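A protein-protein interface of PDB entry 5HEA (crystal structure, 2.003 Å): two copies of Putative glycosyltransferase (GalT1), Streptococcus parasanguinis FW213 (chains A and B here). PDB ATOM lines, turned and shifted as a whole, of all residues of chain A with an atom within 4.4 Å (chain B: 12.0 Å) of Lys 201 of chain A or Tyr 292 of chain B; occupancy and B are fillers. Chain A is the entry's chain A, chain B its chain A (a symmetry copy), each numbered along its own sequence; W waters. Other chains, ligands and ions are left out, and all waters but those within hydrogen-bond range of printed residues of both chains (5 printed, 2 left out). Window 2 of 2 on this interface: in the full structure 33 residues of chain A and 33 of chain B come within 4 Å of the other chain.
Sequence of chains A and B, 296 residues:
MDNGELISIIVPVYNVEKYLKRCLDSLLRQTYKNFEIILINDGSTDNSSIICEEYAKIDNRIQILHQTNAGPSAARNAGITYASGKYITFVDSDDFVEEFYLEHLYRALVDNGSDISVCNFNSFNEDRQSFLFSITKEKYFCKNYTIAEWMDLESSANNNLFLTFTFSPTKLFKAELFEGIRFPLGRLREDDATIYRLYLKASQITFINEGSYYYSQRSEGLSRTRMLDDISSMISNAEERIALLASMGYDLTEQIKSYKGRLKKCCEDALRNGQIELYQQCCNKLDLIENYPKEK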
ATOM      1  N   LEU A 177     -13.069   8.596 -28.435  1.00  0.00           N
ATOM      2  CA  LEU A 177     -13.563   8.921 -27.099  1.00  0.00           C
ATOM      3  C   LEU A 177     -12.562   8.570 -25.975  1.00  0.00           C
ATOM      4  O   LEU A 177     -12.623   9.138 -24.889  1.00  0.00           O
ATOM      5  CB  LEU A 177     -14.884   8.195 -26.833  1.00  0.00           C
ATOM      6  CG  LEU A 177     -16.253   8.745 -27.243  1.00  0.00           C
ATOM      7  CD1 LEU A 177     -16.207   9.989 -28.109  1.00  0.00           C
ATOM      8  CD2 LEU A 177     -17.068   7.662 -27.895  1.00  0.00           C
ATOM      9  N   GLU A 179      -9.407   9.183 -25.563  1.00  0.00           N
ATOM     10  CA  GLU A 179      -8.331  10.136 -25.258  1.00  0.00           C
ATOM     11  C   GLU A 179      -8.345  10.546 -23.780  1.00  0.00           C
ATOM     12  O   GLU A 179      -9.295  11.185 -23.305  1.00  0.00           O
ATOM     13  CB  GLU A 179      -8.416  11.388 -26.139  1.00  0.00           C
ATOM     14  CG  GLU A 179      -7.317  12.413 -25.814  1.00  0.00           C
ATOM     15  CD  GLU A 179      -7.484  13.759 -26.519  1.00  0.00           C
ATOM     16  OE1 GLU A 179      -8.558  14.017 -27.108  1.00  0.00           O
ATOM     17  OE2 GLU A 179      -6.529  14.564 -26.473  1.00  0.00           O
ATOM     18  N   ILE A 181      -8.749   8.743 -21.230  1.00  0.00           N
ATOM     19  CA  ILE A 181      -9.601   7.906 -20.392  1.00  0.00           C
ATOM     20  C   ILE A 181      -9.025   6.501 -20.239  1.00  0.00           C
ATOM     21  O   ILE A 181      -8.828   5.793 -21.233  1.00  0.00           O
ATOM     22  CB  ILE A 181     -11.060   7.833 -20.945  1.00  0.00           C
ATOM     23  CG1 ILE A 181     -11.745   9.204 -20.824  1.00  0.00           C
ATOM     24  CG2 ILE A 181     -11.855   6.806 -20.166  1.00  0.00           C
ATOM     25  CD1 ILE A 181     -13.143   9.267 -21.447  1.00  0.00           C
ATOM     26  N   ARG A 197     -17.519   8.459 -18.004  1.00  0.00           N
ATOM     27  CA  ARG A 197     -16.656   9.484 -18.583  1.00  0.00           C
ATOM     28  C   ARG A 197     -16.645   9.426 -20.115  1.00  0.00           C
ATOM     29  O   ARG A 197     -16.577  10.456 -20.783  1.00  0.00           O
ATOM     30  CB  ARG A 197     -15.246   9.420 -17.992  1.00  0.00           C
ATOM     31  CG  ARG A 197     -15.247   9.645 -16.477  1.00  0.00           C
ATOM     32  CD  ARG A 197     -13.851   9.703 -15.906  1.00  0.00           C
ATOM     33  NE  ARG A 197     -13.348   8.392 -15.494  1.00  0.00           N
ATOM     34  CZ  ARG A 197     -12.181   7.880 -15.886  1.00  0.00           C
ATOM     35  NH1 ARG A 197     -11.409   8.571 -16.722  1.00  0.00           N
ATOM     36  NH2 ARG A 197     -11.773   6.686 -15.439  1.00  0.00           N
ATOM     37  N   LEU A 198     -16.729   8.227 -20.677  1.00  0.00           N
ATOM     38  CA  LEU A 198     -16.904   8.096 -22.126  1.00  0.00           C
ATOM     39  C   LEU A 198     -18.215   8.722 -22.613  1.00  0.00           C
ATOM     40  O   LEU A 198     -18.246   9.417 -23.639  1.00  0.00           O
ATOM     41  CB  LEU A 198     -16.852   6.625 -22.524  1.00  0.00           C
ATOM     42  CG  LEU A 198     -15.491   5.984 -22.277  1.00  0.00           C
ATOM     43  CD1 LEU A 198     -15.631   4.458 -22.278  1.00  0.00           C
ATOM     44  CD2 LEU A 198     -14.522   6.443 -23.368  1.00  0.00           C
ATOM     45  N   TYR A 199     -19.299   8.484 -21.880  1.00  0.00           N
ATOM     46  CA  TYR A 199     -20.587   9.111 -22.210  1.00  0.00           C
ATOM     47  C   TYR A 199     -20.461  10.646 -22.272  1.00  0.00           C
ATOM     48  O   TYR A 199     -20.982  11.313 -23.184  1.00  0.00           O
ATOM     49  CB  TYR A 199     -21.632   8.771 -21.151  1.00  0.00           C
ATOM     50  CG  TYR A 199     -22.045   7.328 -21.021  1.00  0.00           C
ATOM     51  CD1 TYR A 199     -22.050   6.474 -22.111  1.00  0.00           C
ATOM     52  CD2 TYR A 199     -22.472   6.830 -19.789  1.00  0.00           C
ATOM     53  CE1 TYR A 199     -22.446   5.148 -21.972  1.00  0.00           C
ATOM     54  CE2 TYR A 199     -22.862   5.508 -19.639  1.00  0.00           C
ATOM     55  CZ  TYR A 199     -22.847   4.680 -20.729  1.00  0.00           C
ATOM     56  OH  TYR A 199     -23.252   3.386 -20.584  1.00  0.00           O
ATOM     57  N   LEU A 200     -19.761  11.215 -21.297  1.00  0.00           N
ATOM     58  CA  LEU A 200     -19.611  12.676 -21.233  1.00  0.00           C
ATOM     59  C   LEU A 200     -18.815  13.235 -22.421  1.00  0.00           C
ATOM     60  O   LEU A 200     -18.886  14.425 -22.713  1.00  0.00           O
ATOM     61  CB  LEU A 200     -18.985  13.102 -19.897  1.00  0.00           C
ATOM     62  CG  LEU A 200     -19.821  12.845 -18.643  1.00  0.00           C
ATOM     63  CD1 LEU A 200     -18.982  13.042 -17.378  1.00  0.00           C
ATOM     64  CD2 LEU A 200     -21.064  13.750 -18.626  1.00  0.00           C
ATOM     65  N   LYS A 201     -18.068  12.374 -23.113  1.00  0.00           N
ATOM     66  CA  LYS A 201     -17.328  12.787 -24.304  1.00  0.00           C
ATOM     67  C   LYS A 201     -18.237  12.808 -25.530  1.00  0.00           C
ATOM     68  O   LYS A 201     -17.921  13.459 -26.522  1.00  0.00           O
ATOM     69  CB  LYS A 201     -16.153  11.838 -24.572  1.00  0.00           C
ATOM     70  CG  LYS A 201     -14.988  11.936 -23.591  1.00  0.00           C
ATOM     71  CD  LYS A 201     -14.103  13.120 -23.909  1.00  0.00           C
ATOM     72  CE  LYS A 201     -12.668  12.874 -23.450  1.00  0.00           C
ATOM     73  NZ  LYS A 201     -11.890  11.987 -24.363  1.00  0.00           N
ATOM     74  N   ALA A 202     -19.364  12.105 -25.463  1.00  0.00           N
ATOM     75  CA  ALA A 202     -20.222  11.929 -26.641  1.00  0.00           C
ATOM     76  C   ALA A 202     -21.195  13.087 -26.857  1.00  0.00           C
ATOM     77  O   ALA A 202     -21.430  13.883 -25.947  1.00  0.00           O
ATOM     78  CB  ALA A 202     -20.978  10.601 -26.556  1.00  0.00           C
ATOM     79  N   SER A 203     -21.753  13.177 -28.069  1.00  0.00           N
ATOM     80  CA  SER A 203     -22.790  14.165 -28.390  1.00  0.00           C
ATOM     81  C   SER A 203     -24.167  13.515 -28.350  1.00  0.00           C
ATOM     82  O   SER A 203     -25.143  14.129 -27.926  1.00  0.00           O
ATOM     83  CB  SER A 203     -22.569  14.768 -29.786  1.00  0.00           C
ATOM     84  OG  SER A 203     -21.437  15.620 -29.812  1.00  0.00           O
ATOM     85  N   MET A 248     -19.963  20.309 -14.606  1.00  0.00           N
ATOM     86  CA  MET A 248     -20.300  20.406 -16.020  1.00  0.00           C
ATOM     87  C   MET A 248     -21.740  20.857 -16.246  1.00  0.00           C
ATOM     88  O   MET A 248     -22.183  20.988 -17.380  1.00  0.00           O
ATOM     89  CB  MET A 248     -20.047  19.053 -16.695  1.00  0.00           C
ATOM     90  CG  MET A 248     -18.582  18.642 -16.649  1.00  0.00           C
ATOM     91  SD  MET A 248     -18.356  16.908 -17.081  1.00  0.00           S
ATOM     92  CE  MET A 248     -18.917  16.923 -18.775  1.00  0.00           C
ATOM     93  N   LYS B 260     -12.275  23.160  -9.698  1.00  0.00           N
ATOM     94  CA  LYS B 260     -11.625  23.342 -10.996  1.00  0.00           C
ATOM     95  C   LYS B 260     -10.200  23.851 -10.824  1.00  0.00           C
ATOM     96  O   LYS B 260      -9.296  23.425 -11.542  1.00  0.00           O
ATOM     97  CB  LYS B 260     -12.425  24.298 -11.886  1.00  0.00           C
ATOM     98  CG  LYS B 260     -13.794  23.779 -12.264  1.00  0.00           C
ATOM     99  CD  LYS B 260     -14.547  24.739 -13.188  1.00  0.00           C
ATOM    100  CE  LYS B 260     -16.001  24.294 -13.330  1.00  0.00           C
ATOM    101  NZ  LYS B 260     -16.781  24.930 -14.423  1.00  0.00           N
ATOM    102  N   LEU B 263      -8.029  20.839  -9.671  1.00  0.00           N
ATOM    103  CA  LEU B 263      -7.749  19.975 -10.813  1.00  0.00           C
ATOM    104  C   LEU B 263      -6.590  20.509 -11.662  1.00  0.00           C
ATOM    105  O   LEU B 263      -5.715  19.748 -12.086  1.00  0.00           O
ATOM    106  CB  LEU B 263      -9.012  19.812 -11.683  1.00  0.00           C
ATOM    107  CG  LEU B 263     -10.085  18.927 -11.035  1.00  0.00           C
ATOM    108  CD1 LEU B 263     -11.380  18.999 -11.848  1.00  0.00           C
ATOM    109  CD2 LEU B 263      -9.583  17.491 -10.916  1.00  0.00           C
ATOM    110  N   GLN B 280      -3.214  11.532 -15.036  1.00  0.00           N
ATOM    111  CA  GLN B 280      -4.165  11.124 -16.060  1.00  0.00           C
ATOM    112  C   GLN B 280      -5.600  11.442 -15.626  1.00  0.00           C
ATOM    113  O   GLN B 280      -6.385  11.992 -16.407  1.00  0.00           O
ATOM    114  CB  GLN B 280      -3.996   9.626 -16.355  1.00  0.00           C
ATOM    115  CG  GLN B 280      -5.031   9.028 -17.305  1.00  0.00           C
ATOM    116  CD  GLN B 280      -6.134   8.209 -16.599  1.00  0.00           C
ATOM    117  OE1 GLN B 280      -5.872   7.367 -15.730  1.00  0.00           O
ATOM    118  NE2 GLN B 280      -7.380   8.453 -16.996  1.00  0.00           N
ATOM    119  N   GLN B 281      -5.931  11.116 -14.376  1.00  0.00           N
ATOM    120  CA  GLN B 281      -7.293  11.288 -13.880  1.00  0.00           C
ATOM    121  C   GLN B 281      -7.676  12.761 -13.816  1.00  0.00           C
ATOM    122  O   GLN B 281      -8.751  13.152 -14.286  1.00  0.00           O
ATOM    123  CB  GLN B 281      -7.474  10.602 -12.511  1.00  0.00           C
ATOM    124  CG  GLN B 281      -7.516   9.060 -12.588  1.00  0.00           C
ATOM    125  CD  GLN B 281      -8.860   8.515 -13.102  1.00  0.00           C
ATOM    126  OE1 GLN B 281      -9.920   9.129 -12.902  1.00  0.00           O
ATOM    127  NE2 GLN B 281      -8.816   7.351 -13.765  1.00  0.00           N
ATOM    128  N   CYS B 282      -6.788  13.575 -13.246  1.00  0.00           N
ATOM    129  CA  CYS B 282      -7.033  15.009 -13.108  1.00  0.00           C
ATOM    130  C   CYS B 282      -7.102  15.737 -14.436  1.00  0.00           C
ATOM    131  O   CYS B 282      -7.947  16.613 -14.635  1.00  0.00           O
ATOM    132  CB  CYS B 282      -5.943  15.658 -12.249  1.00  0.00           C
ATOM    133  SG  CYS B 282      -6.095  15.265 -10.486  1.00  0.00           S
ATOM    134  N   CYS B 283      -6.188  15.406 -15.340  1.00  0.00           N
ATOM    135  CA  CYS B 283      -6.229  16.016 -16.664  1.00  0.00           C
ATOM    136  C   CYS B 283      -7.476  15.654 -17.432  1.00  0.00           C
ATOM    137  O   CYS B 283      -8.017  16.482 -18.160  1.00  0.00           O
ATOM    138  CB  CYS B 283      -4.992  15.645 -17.479  1.00  0.00           C
ATOM    139  SG  CYS B 283      -3.555  16.513 -16.884  1.00  0.00           S
ATOM    140  N   ASN B 284      -7.934  14.418 -17.284  1.00  0.00           N
ATOM    141  CA  ASN B 284      -9.162  14.002 -17.954  1.00  0.00           C
ATOM    142  C   ASN B 284     -10.365  14.751 -17.397  1.00  0.00           C
ATOM    143  O   ASN B 284     -11.203  15.232 -18.156  1.00  0.00           O
ATOM    144  CB  ASN B 284      -9.360  12.491 -17.841  1.00  0.00           C
ATOM    145  CG  ASN B 284     -10.756  12.045 -18.265  1.00  0.00           C
ATOM    146  OD1 ASN B 284     -11.199  12.297 -19.387  1.00  0.00           O
ATOM    147  ND2 ASN B 284     -11.444  11.361 -17.368  1.00  0.00           N
ATOM    148  N   LYS B 285     -10.434  14.837 -16.069  1.00  0.00           N
ATOM    149  CA  LYS B 285     -11.493  15.566 -15.395  1.00  0.00           C
ATOM    150  C   LYS B 285     -11.506  17.033 -15.825  1.00  0.00           C
ATOM    151  O   LYS B 285     -12.563  17.591 -16.127  1.00  0.00           O
ATOM    152  CB  LYS B 285     -11.380  15.411 -13.862  1.00  0.00           C
ATOM    153  CG  LYS B 285     -11.837  14.035 -13.377  1.00  0.00           C
ATOM    154  CD  LYS B 285     -11.945  13.944 -11.848  1.00  0.00           C
ATOM    155  CE  LYS B 285     -10.847  13.069 -11.260  1.00  0.00           C
ATOM    156  NZ  LYS B 285     -11.050  12.753  -9.805  1.00  0.00           N
ATOM    157  N   LEU B 286     -10.330  17.653 -15.885  1.00  0.00           N
ATOM    158  CA  LEU B 286     -10.244  19.051 -16.308  1.00  0.00           C
ATOM    159  C   LEU B 286     -10.630  19.202 -17.784  1.00  0.00           C
ATOM    160  O   LEU B 286     -11.292  20.164 -18.166  1.00  0.00           O
ATOM    161  CB  LEU B 286      -8.838  19.597 -16.042  1.00  0.00           C
ATOM    162  CG  LEU B 286      -8.598  21.099 -16.203  1.00  0.00           C
ATOM    163  CD1 LEU B 286      -9.438  21.919 -15.220  1.00  0.00           C
ATOM    164  CD2 LEU B 286      -7.109  21.396 -16.041  1.00  0.00           C
ATOM    165  N   ASP B 287     -10.217  18.238 -18.605  1.00  0.00           N
ATOM    166  CA  ASP B 287     -10.591  18.183 -20.013  1.00  0.00           C
ATOM    167  C   ASP B 287     -12.116  18.110 -20.204  1.00  0.00           C
ATOM    168  O   ASP B 287     -12.666  18.767 -21.075  1.00  0.00           O
ATOM    169  CB  ASP B 287      -9.922  16.967 -20.673  1.00  0.00           C
ATOM    170  CG  ASP B 287     -10.180  16.884 -22.173  1.00  0.00           C
ATOM    171  OD1 ASP B 287     -10.353  17.938 -22.822  1.00  0.00           O
ATOM    172  OD2 ASP B 287     -10.195  15.753 -22.706  1.00  0.00           O
ATOM    173  N   LEU B 288     -12.793  17.309 -19.389  1.00  0.00           N
ATOM    174  CA  LEU B 288     -14.243  17.153 -19.508  1.00  0.00           C
ATOM    175  C   LEU B 288     -14.954  18.444 -19.117  1.00  0.00           C
ATOM    176  O   LEU B 288     -15.885  18.891 -19.787  1.00  0.00           O
ATOM    177  CB  LEU B 288     -14.744  16.005 -18.625  1.00  0.00           C
ATOM    178  CG  LEU B 288     -14.387  14.591 -19.078  1.00  0.00           C
ATOM    179  CD1 LEU B 288     -14.853  13.553 -18.057  1.00  0.00           C
ATOM    180  CD2 LEU B 288     -14.996  14.312 -20.446  1.00  0.00           C
ATOM    181  N   ILE B 289     -14.512  19.032 -18.019  1.00  0.00           N
ATOM    182  CA  ILE B 289     -15.159  20.219 -17.482  1.00  0.00           C
ATOM    183  C   ILE B 289     -15.030  21.412 -18.440  1.00  0.00           C
ATOM    184  O   ILE B 289     -16.007  22.122 -18.708  1.00  0.00           O
ATOM    185  CB  ILE B 289     -14.584  20.561 -16.103  1.00  0.00           C
ATOM    186  CG1 ILE B 289     -15.038  19.523 -15.082  1.00  0.00           C
ATOM    187  CG2 ILE B 289     -15.019  21.950 -15.667  1.00  0.00           C
ATOM    188  CD1 ILE B 289     -14.343  19.647 -13.748  1.00  0.00           C
ATOM    189  N   GLU B 290     -13.832  21.603 -18.978  1.00  0.00           N
ATOM    190  CA  GLU B 290     -13.543  22.754 -19.830  1.00  0.00           C
ATOM    191  C   GLU B 290     -13.960  22.568 -21.285  1.00  0.00           C
ATOM    192  O   GLU B 290     -14.325  23.525 -21.955  1.00  0.00           O
ATOM    193  CB  GLU B 290     -12.053  23.108 -19.764  1.00  0.00           C
ATOM    194  CG  GLU B 290     -11.616  23.669 -18.421  1.00  0.00           C
ATOM    195  CD  GLU B 290     -10.167  24.138 -18.422  1.00  0.00           C
ATOM    196  OE1 GLU B 290      -9.422  23.780 -19.365  1.00  0.00           O
ATOM    197  OE2 GLU B 290      -9.773  24.869 -17.481  1.00  0.00           O
ATOM    198  N   ASN B 291     -13.904  21.341 -21.783  1.00  0.00           N
ATOM    199  CA  ASN B 291     -14.117  21.137 -23.207  1.00  0.00           C
ATOM    200  C   ASN B 291     -15.376  20.364 -23.569  1.00  0.00           C
ATOM    201  O   ASN B 291     -15.759  20.316 -24.736  1.00  0.00           O
ATOM    202  CB  ASN B 291     -12.874  20.509 -23.839  1.00  0.00           C
ATOM    203  CG  ASN B 291     -11.646  21.388 -23.672  1.00  0.00           C
ATOM    204  OD1 ASN B 291     -11.723  22.600 -23.858  1.00  0.00           O
ATOM    205  ND2 ASN B 291     -10.519  20.788 -23.289  1.00  0.00           N
ATOM    206  N   TYR B 292     -16.022  19.770 -22.571  1.00  0.00           N
ATOM    207  CA  TYR B 292     -17.260  19.038 -22.821  1.00  0.00           C
ATOM    208  C   TYR B 292     -18.379  19.399 -21.851  1.00  0.00           C
ATOM    209  O   TYR B 292     -19.048  18.507 -21.341  1.00  0.00           O
ATOM    210  CB  TYR B 292     -17.006  17.526 -22.767  1.00  0.00           C
ATOM    211  CG  TYR B 292     -15.943  17.045 -23.729  1.00  0.00           C
ATOM    212  CD1 TYR B 292     -14.594  17.121 -23.397  1.00  0.00           C
ATOM    213  CD2 TYR B 292     -16.286  16.517 -24.969  1.00  0.00           C
ATOM    214  CE1 TYR B 292     -13.613  16.689 -24.276  1.00  0.00           C
ATOM    215  CE2 TYR B 292     -15.311  16.072 -25.856  1.00  0.00           C
ATOM    216  CZ  TYR B 292     -13.978  16.170 -25.504  1.00  0.00           C
ATOM    217  OH  TYR B 292     -12.997  15.729 -26.366  1.00  0.00           O
ATOM    218  N   PRO B 293     -18.609  20.705 -21.602  1.00  0.00           N
ATOM    219  CA  PRO B 293     -19.741  20.990 -20.716  1.00  0.00           C
ATOM    220  C   PRO B 293     -21.071  20.657 -21.398  1.00  0.00           C
ATOM    221  O   PRO B 293     -21.124  20.474 -22.620  1.00  0.00           O
ATOM    222  CB  PRO B 293     -19.630  22.499 -20.491  1.00  0.00           C
ATOM    223  CG  PRO B 293     -19.023  23.007 -21.751  1.00  0.00           C
ATOM    224  CD  PRO B 293     -18.062  21.938 -22.204  1.00  0.00           C
ATOM    225  N   LYS B 294     -22.128  20.568 -20.597  1.00  0.00           N
ATOM    226  CA  LYS B 294     -23.449  20.219 -21.091  1.00  0.00           C
ATOM    227  C   LYS B 294     -23.889  21.170 -22.201  1.00  0.00           C
ATOM    228  O   LYS B 294     -23.588  22.363 -22.150  1.00  0.00           O
ATOM    229  CB  LYS B 294     -24.456  20.264 -19.943  1.00  0.00           C
ATOM    230  CG  LYS B 294     -25.878  19.944 -20.366  1.00  0.00           C
ATOM    231  CD  LYS B 294     -26.876  20.193 -19.246  1.00  0.00           C
ATOM    232  CE  LYS B 294     -28.297  20.164 -19.788  1.00  0.00           C
ATOM    233  NZ  LYS B 294     -29.293  20.033 -18.698  1.00  0.00           N
ATOM    234  N   GLU B 295     -24.582  20.630 -23.204  1.00  0.00           N
ATOM    235  CA  GLU B 295     -25.184  21.447 -24.261  1.00  0.00           C
ATOM    236  C   GLU B 295     -26.568  21.946 -23.856  1.00  0.00           C
ATOM    237  O   GLU B 295     -26.793  23.152 -23.753  1.00  0.00           O
ATOM    238  CB  GLU B 295     -25.287  20.671 -25.577  1.00  0.00           C
ATOM    239  CG  GLU B 295     -23.981  20.559 -26.345  1.00  0.00           C
ATOM    240  CD  GLU B 295     -23.179  19.329 -25.962  1.00  0.00           C
ATOM    241  OE1 GLU B 295     -23.759  18.219 -25.932  1.00  0.00           O
ATOM    242  OE2 GLU B 295     -21.965  19.473 -25.690  1.00  0.00           O
HETATM  243  O   HOH W   1     -10.362  14.427 -25.275  1.00  0.00           O
HETATM  244  O   HOH W   2     -11.085  10.920 -14.670  1.00  0.00           O
HETATM  245  O   HOH W   3     -25.854  15.820 -25.991  1.00  0.00           O
HETATM  246  O   HOH W   4     -20.675  16.392 -21.873  1.00  0.00           O
HETATM  247  O   HOH W   5     -21.141  16.475 -24.698  1.00  0.00           O
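NH2 of Arg 197 of chain A lies close to NE2 of Gln 281 of chain B, 3.5 Å away. The backbone NH (N) of Lys 294 of chain B sits at hydrogen-bond distance from the backbone carbonyl oxygen (O) of Met 248 of chain A, at 3.2 Å. The side-chain amide nitrogen of Asn 284 of chain B sits close to the guanidinium group of Arg 197 of chain A.
The side-chain amide nitrogen (ND2) of Asn 291 of chain B is in hydrogen-bond range of the side-chain carboxylate (OD1) of Asp 287 of chain B, 2.9 Å away. The backbone carbonyl oxygen of Leu 177 of chain A is in hydrogen-bond range of the side-chain amino group of Lys 201 of chain A, 3.0 Å away. The side-chain amino group of Lys 201 of chain A lies within hydrogen-bond range of the backbone carbonyl oxygen of Glu 179 of chain A, at 2.9 Å.
Among the printed residues, merely in contact across the chains: Ile 181 of chain A with Asn 284 of chain B, Leu 200 of chain A with Tyr 292 of chain B, Lys 201 of chain A with Asp 287 of chain B, Lys 201 of chain A with Leu 288 of chain B, Lys 201 of chain A with Tyr 292 of chain B, Met 248 of chain A with Leu 288 of chain B, Met 248 of chain A with Ile 289 of chain B and Met 248 of chain A with Tyr 292 of chain B.
Of chain A, only Leu 200 (3.6 Å), Lys 201 (3.4 Å) and Met 248 (3.0 Å) come within 4 Å of Tyr 292 of chain B. No residue of chain B comes within 4 Å of Leu 177 of chain A. No residue of chain B comes within 4 Å of Leu 198 of chain A. Of chain B, only Tyr 292 comes within 4 Å of Leu 200 of chain A. Ala 202 of chain A touches none of the printed residues of chain B. Printed residues of chain A within 4 Å of Ile 289 of chain B: Met 248. Of the printed residues of chain A, Leu 288 of chain B touches Lys 201 (3.8 Å) and Met 248 (3.8 Å). Of the printed residues of chain A, Gln 281 of chain B touches Arg 197. Of the printed residues of chain B, Arg 197 of chain A touches Gln 281 and Asn 284. Of the printed residues of chain A, Asn 284 of chain B touches Ile 181 and Arg 197. Leu 263 of chain B touches none of the printed residues of chain A. The nearest printed residue of chain A that does not touch Lys 294 of chain B is Leu 200 of chain A (7.2 Å).
Along chain A the printed residues that touch a printed residue of chain B span positions 181 to 248. Of the 18 printed residues of chain B, 7 touch a printed residue of chain A. Among the printed residues, 11 pairs touch across the chains. Among the printed residues, no Asp or Glu carboxylate lies within 4 Å of a Lys or Arg side-chain nitrogen of the other chain.
No position is printed for both chains. Of the 11 pairs that touch across the chains among the printed residues, none has its exchanged pair printed and touching as well.
Water W1 lies within hydrogen-bond range of the side-chain carboxylate (OE1) of Glu 179 of chain A (2.6 Å), the side-chain carboxylate (OD2) of Asp 287 of chain B (2.9 Å), the side-chain amino group (NZ) of Lys 201 of chain A (3.0 Å) and the side-chain hydroxyl (OH) of Tyr 292 of chain B (3.1 Å). Water W3 lies within hydrogen-bond range of the backbone carbonyl oxygen of Ser 203 of chain A (2.7 Å) and the side-chain carboxylate of Glu 295 of chain B (3.2 Å). Water W4 bridges the backbone carbonyl oxygen of Tyr 292 of chain B (2.7 Å) and the backbone carbonyl oxygen of Leu 200 of chain A (2.8 Å). Water W2 lies within hydrogen-bond range of ND2 of Asn 284 of chain B, OE1 of Gln 281 of chain B and NH1 of Arg 197 of chain A. Water W5 bridges O of Ala 202 of chain A (2.9 Å) and OE2 of Glu 295 of chain B (3.3 Å).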
